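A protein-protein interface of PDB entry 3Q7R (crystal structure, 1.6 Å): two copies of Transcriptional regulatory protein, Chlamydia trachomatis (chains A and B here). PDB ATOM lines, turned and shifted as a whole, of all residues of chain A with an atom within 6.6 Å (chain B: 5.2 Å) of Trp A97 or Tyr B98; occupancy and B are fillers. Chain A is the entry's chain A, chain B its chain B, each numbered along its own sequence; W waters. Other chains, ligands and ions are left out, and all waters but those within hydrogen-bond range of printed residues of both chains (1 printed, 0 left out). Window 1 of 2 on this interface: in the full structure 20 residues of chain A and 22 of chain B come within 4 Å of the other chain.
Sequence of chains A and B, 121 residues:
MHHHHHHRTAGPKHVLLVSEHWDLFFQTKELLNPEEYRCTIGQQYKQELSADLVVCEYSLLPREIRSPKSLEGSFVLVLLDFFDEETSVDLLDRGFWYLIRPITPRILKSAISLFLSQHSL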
ATOM      1  N   VAL A  76      -9.643 -12.116  34.189  1.00  0.00           N
ATOM      2  CA  VAL A  76     -10.334 -12.797  33.057  1.00  0.00           C
ATOM      3  C   VAL A  76      -9.346 -13.332  32.030  1.00  0.00           C
ATOM      4  O   VAL A  76      -8.465 -12.582  31.575  1.00  0.00           O
ATOM      5  CB  VAL A  76     -11.323 -11.842  32.360  1.00  0.00           C
ATOM      6  CG1 VAL A  76     -11.957 -12.568  31.153  1.00  0.00           C
ATOM      7  CG2 VAL A  76     -12.466 -11.377  33.336  1.00  0.00           C
ATOM      8  N   LEU A  77      -9.444 -14.628  31.695  1.00  0.00           N
ATOM      9  CA  LEU A  77      -8.632 -15.210  30.627  1.00  0.00           C
ATOM     10  C   LEU A  77      -9.596 -15.547  29.518  1.00  0.00           C
ATOM     11  O   LEU A  77     -10.650 -16.156  29.793  1.00  0.00           O
ATOM     12  CB  LEU A  77      -7.980 -16.518  31.146  1.00  0.00           C
ATOM     13  CG  LEU A  77      -7.255 -17.410  30.111  1.00  0.00           C
ATOM     14  CD1 LEU A  77      -5.984 -16.724  29.625  1.00  0.00           C
ATOM     15  CD2 LEU A  77      -6.891 -18.746  30.778  1.00  0.00           C
ATOM     16  N   VAL A  78      -9.243 -15.198  28.288  1.00  0.00           N
ATOM     17  CA  VAL A  78     -10.180 -15.340  27.165  1.00  0.00           C
ATOM     18  C   VAL A  78      -9.811 -16.531  26.273  1.00  0.00           C
ATOM     19  O   VAL A  78      -8.636 -16.787  26.028  1.00  0.00           O
ATOM     20  CB  VAL A  78     -10.185 -14.037  26.357  1.00  0.00           C
ATOM     21  CG1 VAL A  78     -10.941 -14.221  25.049  1.00  0.00           C
ATOM     22  CG2 VAL A  78     -10.740 -12.903  27.201  1.00  0.00           C
ATOM     23  N   LEU A  79     -10.815 -17.288  25.821  1.00  0.00           N
ATOM     24  CA  LEU A  79     -10.580 -18.418  24.924  1.00  0.00           C
ATOM     25  C   LEU A  79     -11.049 -18.049  23.521  1.00  0.00           C
ATOM     26  O   LEU A  79     -12.223 -17.724  23.318  1.00  0.00           O
ATOM     27  CB  LEU A  79     -11.341 -19.657  25.368  1.00  0.00           C
ATOM     28  CG  LEU A  79     -11.142 -20.057  26.823  1.00  0.00           C
ATOM     29  CD1 LEU A  79     -11.894 -21.436  27.059  1.00  0.00           C
ATOM     30  CD2 LEU A  79      -9.621 -20.144  27.133  1.00  0.00           C
ATOM     31  N   LEU A  91      -7.810  -7.416  22.298  1.00  0.00           N
ATOM     32  CA  LEU A  91      -7.916  -8.122  23.593  1.00  0.00           C
ATOM     33  C   LEU A  91      -6.804  -7.687  24.524  1.00  0.00           C
ATOM     34  O   LEU A  91      -7.051  -7.339  25.701  1.00  0.00           O
ATOM     35  CB  LEU A  91      -7.828  -9.646  23.448  1.00  0.00           C
ATOM     36  CG  LEU A  91      -9.139 -10.292  22.978  1.00  0.00           C
ATOM     37  CD1 LEU A  91      -8.852 -11.765  22.618  1.00  0.00           C
ATOM     38  CD2 LEU A  91     -10.294 -10.200  24.046  1.00  0.00           C
ATOM     39  N   LEU A  92      -5.584  -7.666  24.006  1.00  0.00           N
ATOM     40  CA  LEU A  92      -4.438  -7.362  24.863  1.00  0.00           C
ATOM     41  C   LEU A  92      -4.539  -5.909  25.381  1.00  0.00           C
ATOM     42  O   LEU A  92      -4.257  -5.610  26.554  1.00  0.00           O
ATOM     43  CB  LEU A  92      -3.151  -7.557  24.084  1.00  0.00           C
ATOM     44  CG  LEU A  92      -2.891  -9.031  23.680  1.00  0.00           C
ATOM     45  CD1 LEU A  92      -1.792  -9.062  22.567  1.00  0.00           C
ATOM     46  CD2 LEU A  92      -2.458  -9.908  24.902  1.00  0.00           C
ATOM     47  N   GLY A  95      -6.752  -5.444  28.244  1.00  0.00           N
ATOM     48  CA  GLY A  95      -6.318  -6.094  29.477  1.00  0.00           C
ATOM     49  C   GLY A  95      -6.520  -7.573  29.574  1.00  0.00           C
ATOM     50  O   GLY A  95      -6.295  -8.159  30.651  1.00  0.00           O
ATOM     51  N   PHE A  96      -6.853  -8.215  28.456  1.00  0.00           N
ATOM     52  CA  PHE A  96      -7.128  -9.655  28.495  1.00  0.00           C
ATOM     53  C   PHE A  96      -6.019 -10.476  27.807  1.00  0.00           C
ATOM     54  O   PHE A  96      -5.803 -10.345  26.589  1.00  0.00           O
ATOM     55  CB  PHE A  96      -8.409  -9.942  27.711  1.00  0.00           C
ATOM     56  CG  PHE A  96      -9.617  -9.238  28.275  1.00  0.00           C
ATOM     57  CD1 PHE A  96     -10.175  -9.658  29.470  1.00  0.00           C
ATOM     58  CD2 PHE A  96     -10.214  -8.175  27.589  1.00  0.00           C
ATOM     59  CE1 PHE A  96     -11.326  -9.001  29.986  1.00  0.00           C
ATOM     60  CE2 PHE A  96     -11.356  -7.543  28.114  1.00  0.00           C
ATOM     61  CZ  PHE A  96     -11.879  -7.958  29.339  1.00  0.00           C
ATOM     62  N   TRP A  97      -5.438 -11.388  28.574  1.00  0.00           N
ATOM     63  CA  TRP A  97      -4.627 -12.428  27.996  1.00  0.00           C
ATOM     64  C   TRP A  97      -5.561 -13.512  27.410  1.00  0.00           C
ATOM     65  O   TRP A  97      -6.751 -13.577  27.766  1.00  0.00           O
ATOM     66  CB  TRP A  97      -3.663 -13.021  29.078  1.00  0.00           C
ATOM     67  CG  TRP A  97      -2.703 -14.062  28.560  1.00  0.00           C
ATOM     68  CD1 TRP A  97      -2.537 -15.349  29.022  1.00  0.00           C
ATOM     69  CD2 TRP A  97      -1.768 -13.913  27.493  1.00  0.00           C
ATOM     70  NE1 TRP A  97      -1.559 -16.013  28.287  1.00  0.00           N
ATOM     71  CE2 TRP A  97      -1.061 -15.160  27.351  1.00  0.00           C
ATOM     72  CE3 TRP A  97      -1.455 -12.863  26.644  1.00  0.00           C
ATOM     73  CZ2 TRP A  97      -0.092 -15.371  26.382  1.00  0.00           C
ATOM     74  CZ3 TRP A  97      -0.448 -13.079  25.655  1.00  0.00           C
ATOM     75  CH2 TRP A  97       0.202 -14.333  25.543  1.00  0.00           C
ATOM     76  N   TYR A  98      -5.026 -14.371  26.534  1.00  0.00           N
ATOM     77  CA  TYR A  98      -5.920 -15.308  25.824  1.00  0.00           C
ATOM     78  C   TYR A  98      -5.161 -16.552  25.394  1.00  0.00           C
ATOM     79  O   TYR A  98      -3.916 -16.540  25.365  1.00  0.00           O
ATOM     80  CB  TYR A  98      -6.568 -14.676  24.539  1.00  0.00           C
ATOM     81  CG  TYR A  98      -5.541 -14.139  23.565  1.00  0.00           C
ATOM     82  CD1 TYR A  98      -4.909 -14.968  22.675  1.00  0.00           C
ATOM     83  CD2 TYR A  98      -5.207 -12.776  23.576  1.00  0.00           C
ATOM     84  CE1 TYR A  98      -3.949 -14.455  21.776  1.00  0.00           C
ATOM     85  CE2 TYR A  98      -4.256 -12.252  22.711  1.00  0.00           C
ATOM     86  CZ  TYR A  98      -3.615 -13.094  21.852  1.00  0.00           C
ATOM     87  OH  TYR A  98      -2.637 -12.605  20.965  1.00  0.00           O
ATOM     88  N   LEU A  99      -5.912 -17.618  25.149  1.00  0.00           N
ATOM     89  CA  LEU A  99      -5.414 -18.829  24.476  1.00  0.00           C
ATOM     90  C   LEU A  99      -6.204 -18.929  23.188  1.00  0.00           C
ATOM     91  O   LEU A  99      -7.422 -18.627  23.189  1.00  0.00           O
ATOM     92  CB  LEU A  99      -5.734 -20.099  25.287  1.00  0.00           C
ATOM     93  CG  LEU A  99      -5.067 -20.171  26.661  1.00  0.00           C
ATOM     94  CD1 LEU A  99      -5.584 -21.362  27.475  1.00  0.00           C
ATOM     95  CD2 LEU A  99      -3.567 -20.301  26.408  1.00  0.00           C
ATOM     96  N   ILE A 100      -5.577 -19.427  22.112  1.00  0.00           N
ATOM     97  CA  ILE A 100      -6.260 -19.649  20.844  1.00  0.00           C
ATOM     98  C   ILE A 100      -6.347 -21.152  20.643  1.00  0.00           C
ATOM     99  O   ILE A 100      -5.368 -21.885  20.934  1.00  0.00           O
ATOM    100  CB  ILE A 100      -5.543 -18.981  19.673  1.00  0.00           C
ATOM    101  CG1 ILE A 100      -5.472 -17.461  19.937  1.00  0.00           C
ATOM    102  CG2 ILE A 100      -6.264 -19.341  18.339  1.00  0.00           C
ATOM    103  CD1 ILE A 100      -4.920 -16.617  18.731  1.00  0.00           C
ATOM    104  N   PRO A 102      -6.405 -24.865  19.011  1.00  0.00           N
ATOM    105  CA  PRO A 102      -6.990 -25.864  19.916  1.00  0.00           C
ATOM    106  C   PRO A 102      -6.675 -25.696  21.381  1.00  0.00           C
ATOM    107  O   PRO A 102      -5.544 -25.380  21.776  1.00  0.00           O
ATOM    108  CB  PRO A 102      -6.357 -27.198  19.443  1.00  0.00           C
ATOM    109  CG  PRO A 102      -5.986 -26.946  18.065  1.00  0.00           C
ATOM    110  CD  PRO A 102      -5.600 -25.495  17.940  1.00  0.00           C
ATOM    111  N   ILE A 107      -4.420 -28.498  28.430  1.00  0.00           N
ATOM    112  CA  ILE A 107      -3.913 -27.127  28.285  1.00  0.00           C
ATOM    113  C   ILE A 107      -4.659 -26.207  29.208  1.00  0.00           C
ATOM    114  O   ILE A 107      -4.047 -25.362  29.851  1.00  0.00           O
ATOM    115  CB  ILE A 107      -4.058 -26.685  26.864  1.00  0.00           C
ATOM    116  CG1 ILE A 107      -3.057 -27.487  26.019  1.00  0.00           C
ATOM    117  CG2 ILE A 107      -3.841 -25.154  26.726  1.00  0.00           C
ATOM    118  CD1 ILE A 107      -3.164 -27.249  24.537  1.00  0.00           C
ATOM    119  N   PHE A 115      -1.956 -19.239  35.613  1.00  0.00           N
ATOM    120  CA  PHE A 115      -2.491 -17.896  35.785  1.00  0.00           C
ATOM    121  C   PHE A 115      -2.696 -17.578  37.258  1.00  0.00           C
ATOM    122  O   PHE A 115      -2.304 -16.509  37.751  1.00  0.00           O
ATOM    123  CB  PHE A 115      -3.820 -17.785  35.021  1.00  0.00           C
ATOM    124  CG  PHE A 115      -4.284 -16.363  34.828  1.00  0.00           C
ATOM    125  CD1 PHE A 115      -4.321 -15.820  33.561  1.00  0.00           C
ATOM    126  CD2 PHE A 115      -4.661 -15.582  35.905  1.00  0.00           C
ATOM    127  CE1 PHE A 115      -4.738 -14.488  33.362  1.00  0.00           C
ATOM    128  CE2 PHE A 115      -5.054 -14.254  35.710  1.00  0.00           C
ATOM    129  CZ  PHE A 115      -5.083 -13.713  34.456  1.00  0.00           C
ATOM    130  N   LEU B  77       7.980 -14.644  28.107  1.00  0.00           N
ATOM    131  CA  LEU B  77       6.951 -15.032  27.146  1.00  0.00           C
ATOM    132  C   LEU B  77       7.662 -15.793  26.043  1.00  0.00           C
ATOM    133  O   LEU B  77       8.682 -15.321  25.568  1.00  0.00           O
ATOM    134  CB  LEU B  77       6.296 -13.798  26.552  1.00  0.00           C
ATOM    135  CG  LEU B  77       5.366 -14.009  25.350  1.00  0.00           C
ATOM    136  CD1 LEU B  77       4.126 -14.847  25.741  1.00  0.00           C
ATOM    137  CD2 LEU B  77       4.993 -12.632  24.694  1.00  0.00           C
ATOM    138  N   VAL B  78       7.119 -16.945  25.638  1.00  0.00           N
ATOM    139  CA  VAL B  78       7.781 -17.815  24.652  1.00  0.00           C
ATOM    140  C   VAL B  78       7.049 -17.699  23.323  1.00  0.00           C
ATOM    141  O   VAL B  78       5.836 -17.665  23.309  1.00  0.00           O
ATOM    142  CB  VAL B  78       7.789 -19.292  25.155  1.00  0.00           C
ATOM    143  CG1 VAL B  78       8.289 -20.238  24.057  1.00  0.00           C
ATOM    144  CG2 VAL B  78       8.659 -19.410  26.417  1.00  0.00           C
ATOM    145  N   LEU B  79       7.782 -17.638  22.218  1.00  0.00           N
ATOM    146  CA  LEU B  79       7.183 -17.587  20.885  1.00  0.00           C
ATOM    147  C   LEU B  79       7.312 -18.953  20.206  1.00  0.00           C
ATOM    148  O   LEU B  79       8.404 -19.527  20.166  1.00  0.00           O
ATOM    149  CB  LEU B  79       7.892 -16.501  20.044  1.00  0.00           C
ATOM    150  CG  LEU B  79       8.045 -15.125  20.692  1.00  0.00           C
ATOM    151  CD1 LEU B  79       8.623 -14.074  19.701  1.00  0.00           C
ATOM    152  CD2 LEU B  79       6.688 -14.608  21.254  1.00  0.00           C
ATOM    153  N   LEU B  80       6.207 -19.473  19.669  1.00  0.00           N
ATOM    154  CA  LEU B  80       6.190 -20.809  19.062  1.00  0.00           C
ATOM    155  C   LEU B  80       5.843 -20.691  17.596  1.00  0.00           C
ATOM    156  O   LEU B  80       4.962 -19.917  17.240  1.00  0.00           O
ATOM    157  CB  LEU B  80       5.105 -21.683  19.709  1.00  0.00           C
ATOM    158  CG  LEU B  80       5.444 -22.255  21.084  1.00  0.00           C
ATOM    159  CD1 LEU B  80       4.169 -22.757  21.711  1.00  0.00           C
ATOM    160  CD2 LEU B  80       6.467 -23.359  20.959  1.00  0.00           C
ATOM    161  N   SER B  88       2.826 -27.248  24.484  1.00  0.00           N
ATOM    162  CA  SER B  88       2.049 -26.234  25.203  1.00  0.00           C
ATOM    163  C   SER B  88       1.919 -26.587  26.679  1.00  0.00           C
ATOM    164  O   SER B  88       2.118 -25.739  27.555  1.00  0.00           O
ATOM    165  CB  SER B  88       0.642 -26.088  24.622  1.00  0.00           C
ATOM    166  OG  SER B  88       0.670 -25.504  23.340  1.00  0.00           O
ATOM    167  N   LEU B  91       5.236 -26.197  28.528  1.00  0.00           N
ATOM    168  CA  LEU B  91       5.646 -24.807  28.743  1.00  0.00           C
ATOM    169  C   LEU B  91       4.860 -24.197  29.884  1.00  0.00           C
ATOM    170  O   LEU B  91       5.423 -23.541  30.750  1.00  0.00           O
ATOM    171  CB  LEU B  91       5.374 -23.957  27.484  1.00  0.00           C
ATOM    172  CG  LEU B  91       6.447 -24.113  26.384  1.00  0.00           C
ATOM    173  CD1 LEU B  91       6.003 -23.321  25.130  1.00  0.00           C
ATOM    174  CD2 LEU B  91       7.837 -23.660  26.886  1.00  0.00           C
ATOM    175  N   LEU B  92       3.546 -24.400  29.875  1.00  0.00           N
ATOM    176  CA  LEU B  92       2.714 -23.822  30.937  1.00  0.00           C
ATOM    177  C   LEU B  92       3.109 -24.390  32.314  1.00  0.00           C
ATOM    178  O   LEU B  92       3.193 -23.658  33.299  1.00  0.00           O
ATOM    179  CB  LEU B  92       1.222 -24.090  30.693  1.00  0.00           C
ATOM    180  CG  LEU B  92       0.679 -23.401  29.426  1.00  0.00           C
ATOM    181  CD1 LEU B  92      -0.653 -24.034  28.965  1.00  0.00           C
ATOM    182  CD2 LEU B  92       0.585 -21.892  29.588  1.00  0.00           C
ATOM    183  N   PHE B  96       5.833 -20.905  31.782  1.00  0.00           N
ATOM    184  CA  PHE B  96       5.905 -20.025  30.607  1.00  0.00           C
ATOM    185  C   PHE B  96       4.579 -19.824  29.856  1.00  0.00           C
ATOM    186  O   PHE B  96       4.016 -20.792  29.365  1.00  0.00           O
ATOM    187  CB  PHE B  96       6.888 -20.596  29.579  1.00  0.00           C
ATOM    188  CG  PHE B  96       8.288 -20.729  30.094  1.00  0.00           C
ATOM    189  CD1 PHE B  96       9.132 -19.637  30.135  1.00  0.00           C
ATOM    190  CD2 PHE B  96       8.756 -21.961  30.544  1.00  0.00           C
ATOM    191  CE1 PHE B  96      10.440 -19.758  30.617  1.00  0.00           C
ATOM    192  CE2 PHE B  96      10.076 -22.094  31.035  1.00  0.00           C
ATOM    193  CZ  PHE B  96      10.903 -20.994  31.072  1.00  0.00           C
ATOM    194  N   TRP B  97       4.122 -18.585  29.711  1.00  0.00           N
ATOM    195  CA  TRP B  97       3.091 -18.307  28.698  1.00  0.00           C
ATOM    196  C   TRP B  97       3.682 -18.271  27.293  1.00  0.00           C
ATOM    197  O   TRP B  97       4.914 -18.124  27.129  1.00  0.00           O
ATOM    198  CB  TRP B  97       2.439 -16.951  28.938  1.00  0.00           C
ATOM    199  CG  TRP B  97       1.689 -16.930  30.171  1.00  0.00           C
ATOM    200  CD1 TRP B  97       2.049 -16.314  31.320  1.00  0.00           C
ATOM    201  CD2 TRP B  97       0.428 -17.595  30.440  1.00  0.00           C
ATOM    202  NE1 TRP B  97       1.099 -16.539  32.293  1.00  0.00           N
ATOM    203  CE2 TRP B  97       0.086 -17.306  31.777  1.00  0.00           C
ATOM    204  CE3 TRP B  97      -0.423 -18.395  29.686  1.00  0.00           C
ATOM    205  CZ2 TRP B  97      -1.087 -17.798  32.385  1.00  0.00           C
ATOM    206  CZ3 TRP B  97      -1.619 -18.843  30.261  1.00  0.00           C
ATOM    207  CH2 TRP B  97      -1.920 -18.572  31.613  1.00  0.00           C
ATOM    208  N   TYR B  98       2.833 -18.376  26.273  1.00  0.00           N
ATOM    209  CA  TYR B  98       3.340 -18.339  24.893  1.00  0.00           C
ATOM    210  C   TYR B  98       2.375 -17.681  23.895  1.00  0.00           C
ATOM    211  O   TYR B  98       1.150 -17.543  24.148  1.00  0.00           O
ATOM    212  CB  TYR B  98       3.630 -19.777  24.410  1.00  0.00           C
ATOM    213  CG  TYR B  98       2.452 -20.720  24.556  1.00  0.00           C
ATOM    214  CD1 TYR B  98       1.439 -20.732  23.614  1.00  0.00           C
ATOM    215  CD2 TYR B  98       2.346 -21.578  25.652  1.00  0.00           C
ATOM    216  CE1 TYR B  98       0.352 -21.561  23.741  1.00  0.00           C
ATOM    217  CE2 TYR B  98       1.268 -22.431  25.789  1.00  0.00           C
ATOM    218  CZ  TYR B  98       0.262 -22.406  24.835  1.00  0.00           C
ATOM    219  OH  TYR B  98      -0.836 -23.220  24.915  1.00  0.00           O
ATOM    220  N   LEU B  99       2.924 -17.298  22.752  1.00  0.00           N
ATOM    221  CA  LEU B  99       2.129 -17.020  21.561  1.00  0.00           C
ATOM    222  C   LEU B  99       2.544 -17.952  20.469  1.00  0.00           C
ATOM    223  O   LEU B  99       3.725 -18.295  20.365  1.00  0.00           O
ATOM    224  CB  LEU B  99       2.358 -15.617  21.055  1.00  0.00           C
ATOM    225  CG  LEU B  99       1.899 -14.575  22.038  1.00  0.00           C
ATOM    226  CD1 LEU B  99       2.386 -13.211  21.562  1.00  0.00           C
ATOM    227  CD2 LEU B  99       0.347 -14.678  22.063  1.00  0.00           C
ATOM    228  N   ILE B 100       1.578 -18.347  19.647  1.00  0.00           N
ATOM    229  CA  ILE B 100       1.869 -19.188  18.498  1.00  0.00           C
ATOM    230  C   ILE B 100       1.717 -18.349  17.234  1.00  0.00           C
ATOM    231  O   ILE B 100       0.774 -17.567  17.112  1.00  0.00           O
ATOM    232  CB  ILE B 100       0.946 -20.428  18.483  1.00  0.00           C
ATOM    233  CG1 ILE B 100       1.244 -21.302  19.718  1.00  0.00           C
ATOM    234  CG2 ILE B 100       1.220 -21.294  17.248  1.00  0.00           C
ATOM    235  CD1 ILE B 100       0.213 -22.348  20.000  1.00  0.00           C
ATOM    236  N   ALA B 111       1.384  -7.267  23.730  1.00  0.00           N
ATOM    237  CA  ALA B 111       1.664  -8.298  24.744  1.00  0.00           C
ATOM    238  C   ALA B 111       2.733  -7.863  25.740  1.00  0.00           C
ATOM    239  O   ALA B 111       2.574  -8.043  26.945  1.00  0.00           O
ATOM    240  CB  ALA B 111       2.098  -9.601  24.067  1.00  0.00           C
ATOM    241  N   LEU B 114       1.024  -5.411  28.076  1.00  0.00           N
ATOM    242  CA  LEU B 114       0.114  -6.016  29.023  1.00  0.00           C
ATOM    243  C   LEU B 114       0.957  -6.719  30.130  1.00  0.00           C
ATOM    244  O   LEU B 114       0.666  -6.579  31.333  1.00  0.00           O
ATOM    245  CB  LEU B 114      -0.783  -7.020  28.276  1.00  0.00           C
ATOM    246  CG  LEU B 114      -1.743  -7.745  29.233  1.00  0.00           C
ATOM    247  CD1 LEU B 114      -2.714  -6.776  29.943  1.00  0.00           C
ATOM    248  CD2 LEU B 114      -2.561  -8.762  28.427  1.00  0.00           C
ATOM    249  N   PHE B 115       1.989  -7.462  29.741  1.00  0.00           N
ATOM    250  CA  PHE B 115       2.781  -8.238  30.725  1.00  0.00           C
ATOM    251  C   PHE B 115       3.401  -7.291  31.740  1.00  0.00           C
ATOM    252  O   PHE B 115       3.350  -7.539  32.922  1.00  0.00           O
ATOM    253  CB  PHE B 115       3.869  -9.085  30.058  1.00  0.00           C
ATOM    254  CG  PHE B 115       3.399 -10.437  29.614  1.00  0.00           C
ATOM    255  CD1 PHE B 115       2.290 -10.554  28.796  1.00  0.00           C
ATOM    256  CD2 PHE B 115       4.084 -11.596  30.005  1.00  0.00           C
ATOM    257  CE1 PHE B 115       1.846 -11.789  28.377  1.00  0.00           C
ATOM    258  CE2 PHE B 115       3.654 -12.838  29.595  1.00  0.00           C
ATOM    259  CZ  PHE B 115       2.526 -12.939  28.769  1.00  0.00           C
HETATM  260  O   HOH W   1      -1.606 -18.005  24.565  1.00  0.00           O
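Leu A92 touches Leu B114 (CD2 to CD2, 3.7 Å).
CD1 of Leu B114 touches CA of Gly A95, at 3.7 Å.
Phe A96 touches Leu B114.
CH2 of Trp A97 touches CD1 of Leu B77, 3.96 Å away.
Trp A97 touches Trp B97.
Leu B114 touches Trp A97 (CD2 to N, 3.9 Å).
Phe B115 touches Trp A97 (CE1 to CZ3, 3.8 Å).
OH of Tyr A98 touches CD2 of Leu B99, at 3.8 Å.
Ser B88 touches Ile A107.
Phe A115 touches Trp B97.
Printed residues of chain B that touch a printed residue of chain A: Leu B77, Ser B88, Leu B92, Trp B97, Tyr B98, Leu B99, Ala B111, Leu B114 and Phe B115.
Hydrophobic or aromatic side chains of chain B within 4 Å of the printed part of chain A: Leu B77, Leu B92, Trp B97, Leu B99, Leu B114 and Phe B115.
Among the printed residues, 14 pairs touch across the chains.
The backbone NH (N) of Leu B80 sits at hydrogen-bond distance from the backbone carbonyl oxygen (O) of Leu B99, at 2.8 Å.
O of Leu A91 is in hydrogen-bond range of N of Phe A96 (2.9 Å).
The side-chain hydroxyl (OG) of Ser B88 is in hydrogen-bond range of the side-chain hydroxyl (OH) of Tyr B98.
The backbone carbonyl oxygen (O) of Val B78 is in hydrogen-bond range of the backbone NH (N) of Leu B99, at 3.0 Å.
The backbone carbonyl oxygen (O) of Trp A97 is in hydrogen-bond range of the backbone NH (N) of Val A78.
The backbone carbonyl oxygen (O) of Trp B97 lies within hydrogen-bond range of the backbone NH (N) of Val B78.
Of the printed residues of chain B, Phe A96 touches Leu B114.
Trp A97 touches just these residues of chain B: Leu B77, Trp B97, Tyr B98, Leu B99, Leu B114 and Phe B115.
Printed residues of chain B within 4 Å of Phe A115: Trp B97 (3.6 Å).
Val B78 touches none of the printed residues of chain A.
Printed residues of chain A within 4 Å of Tyr B98: Trp A97 (3.4 Å).
Printed residues of chain A within 4 Å of Leu B99: Trp A97 (3.5 Å) and Tyr A98 (3.8 Å).
Of the printed residues of chain A, Leu B114 touches Leu A92, Gly A95, Phe A96 and Trp A97.
The nearest residue of chain B that does not touch Trp A97 is Ala B111 (4.6 Å).
The nearest printed residue of chain A that does not touch Tyr B98 is Ile A107 (4.01 Å).
The nearest printed residue of chain B that does not touch Gly A95 is Phe B115 (8.4 Å).
Trp A97 touches Leu B77, but with the chains exchanged Leu A77 does not touch Trp B97 (4.9 Å).
Trp A97 touches its own counterpart, Trp B97.
Trp A97 touches Leu B99, but with the chains exchanged Leu A99 does not touch Trp B97 (4.6 Å).
Tyr A98 touches Leu B99, but with the chains exchanged Leu A99 does not touch Tyr B98 (4.3 Å).
11 positions are printed for both chains.
Water W1 lies within hydrogen-bond range of O of Tyr B98 and O of Tyr A98.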
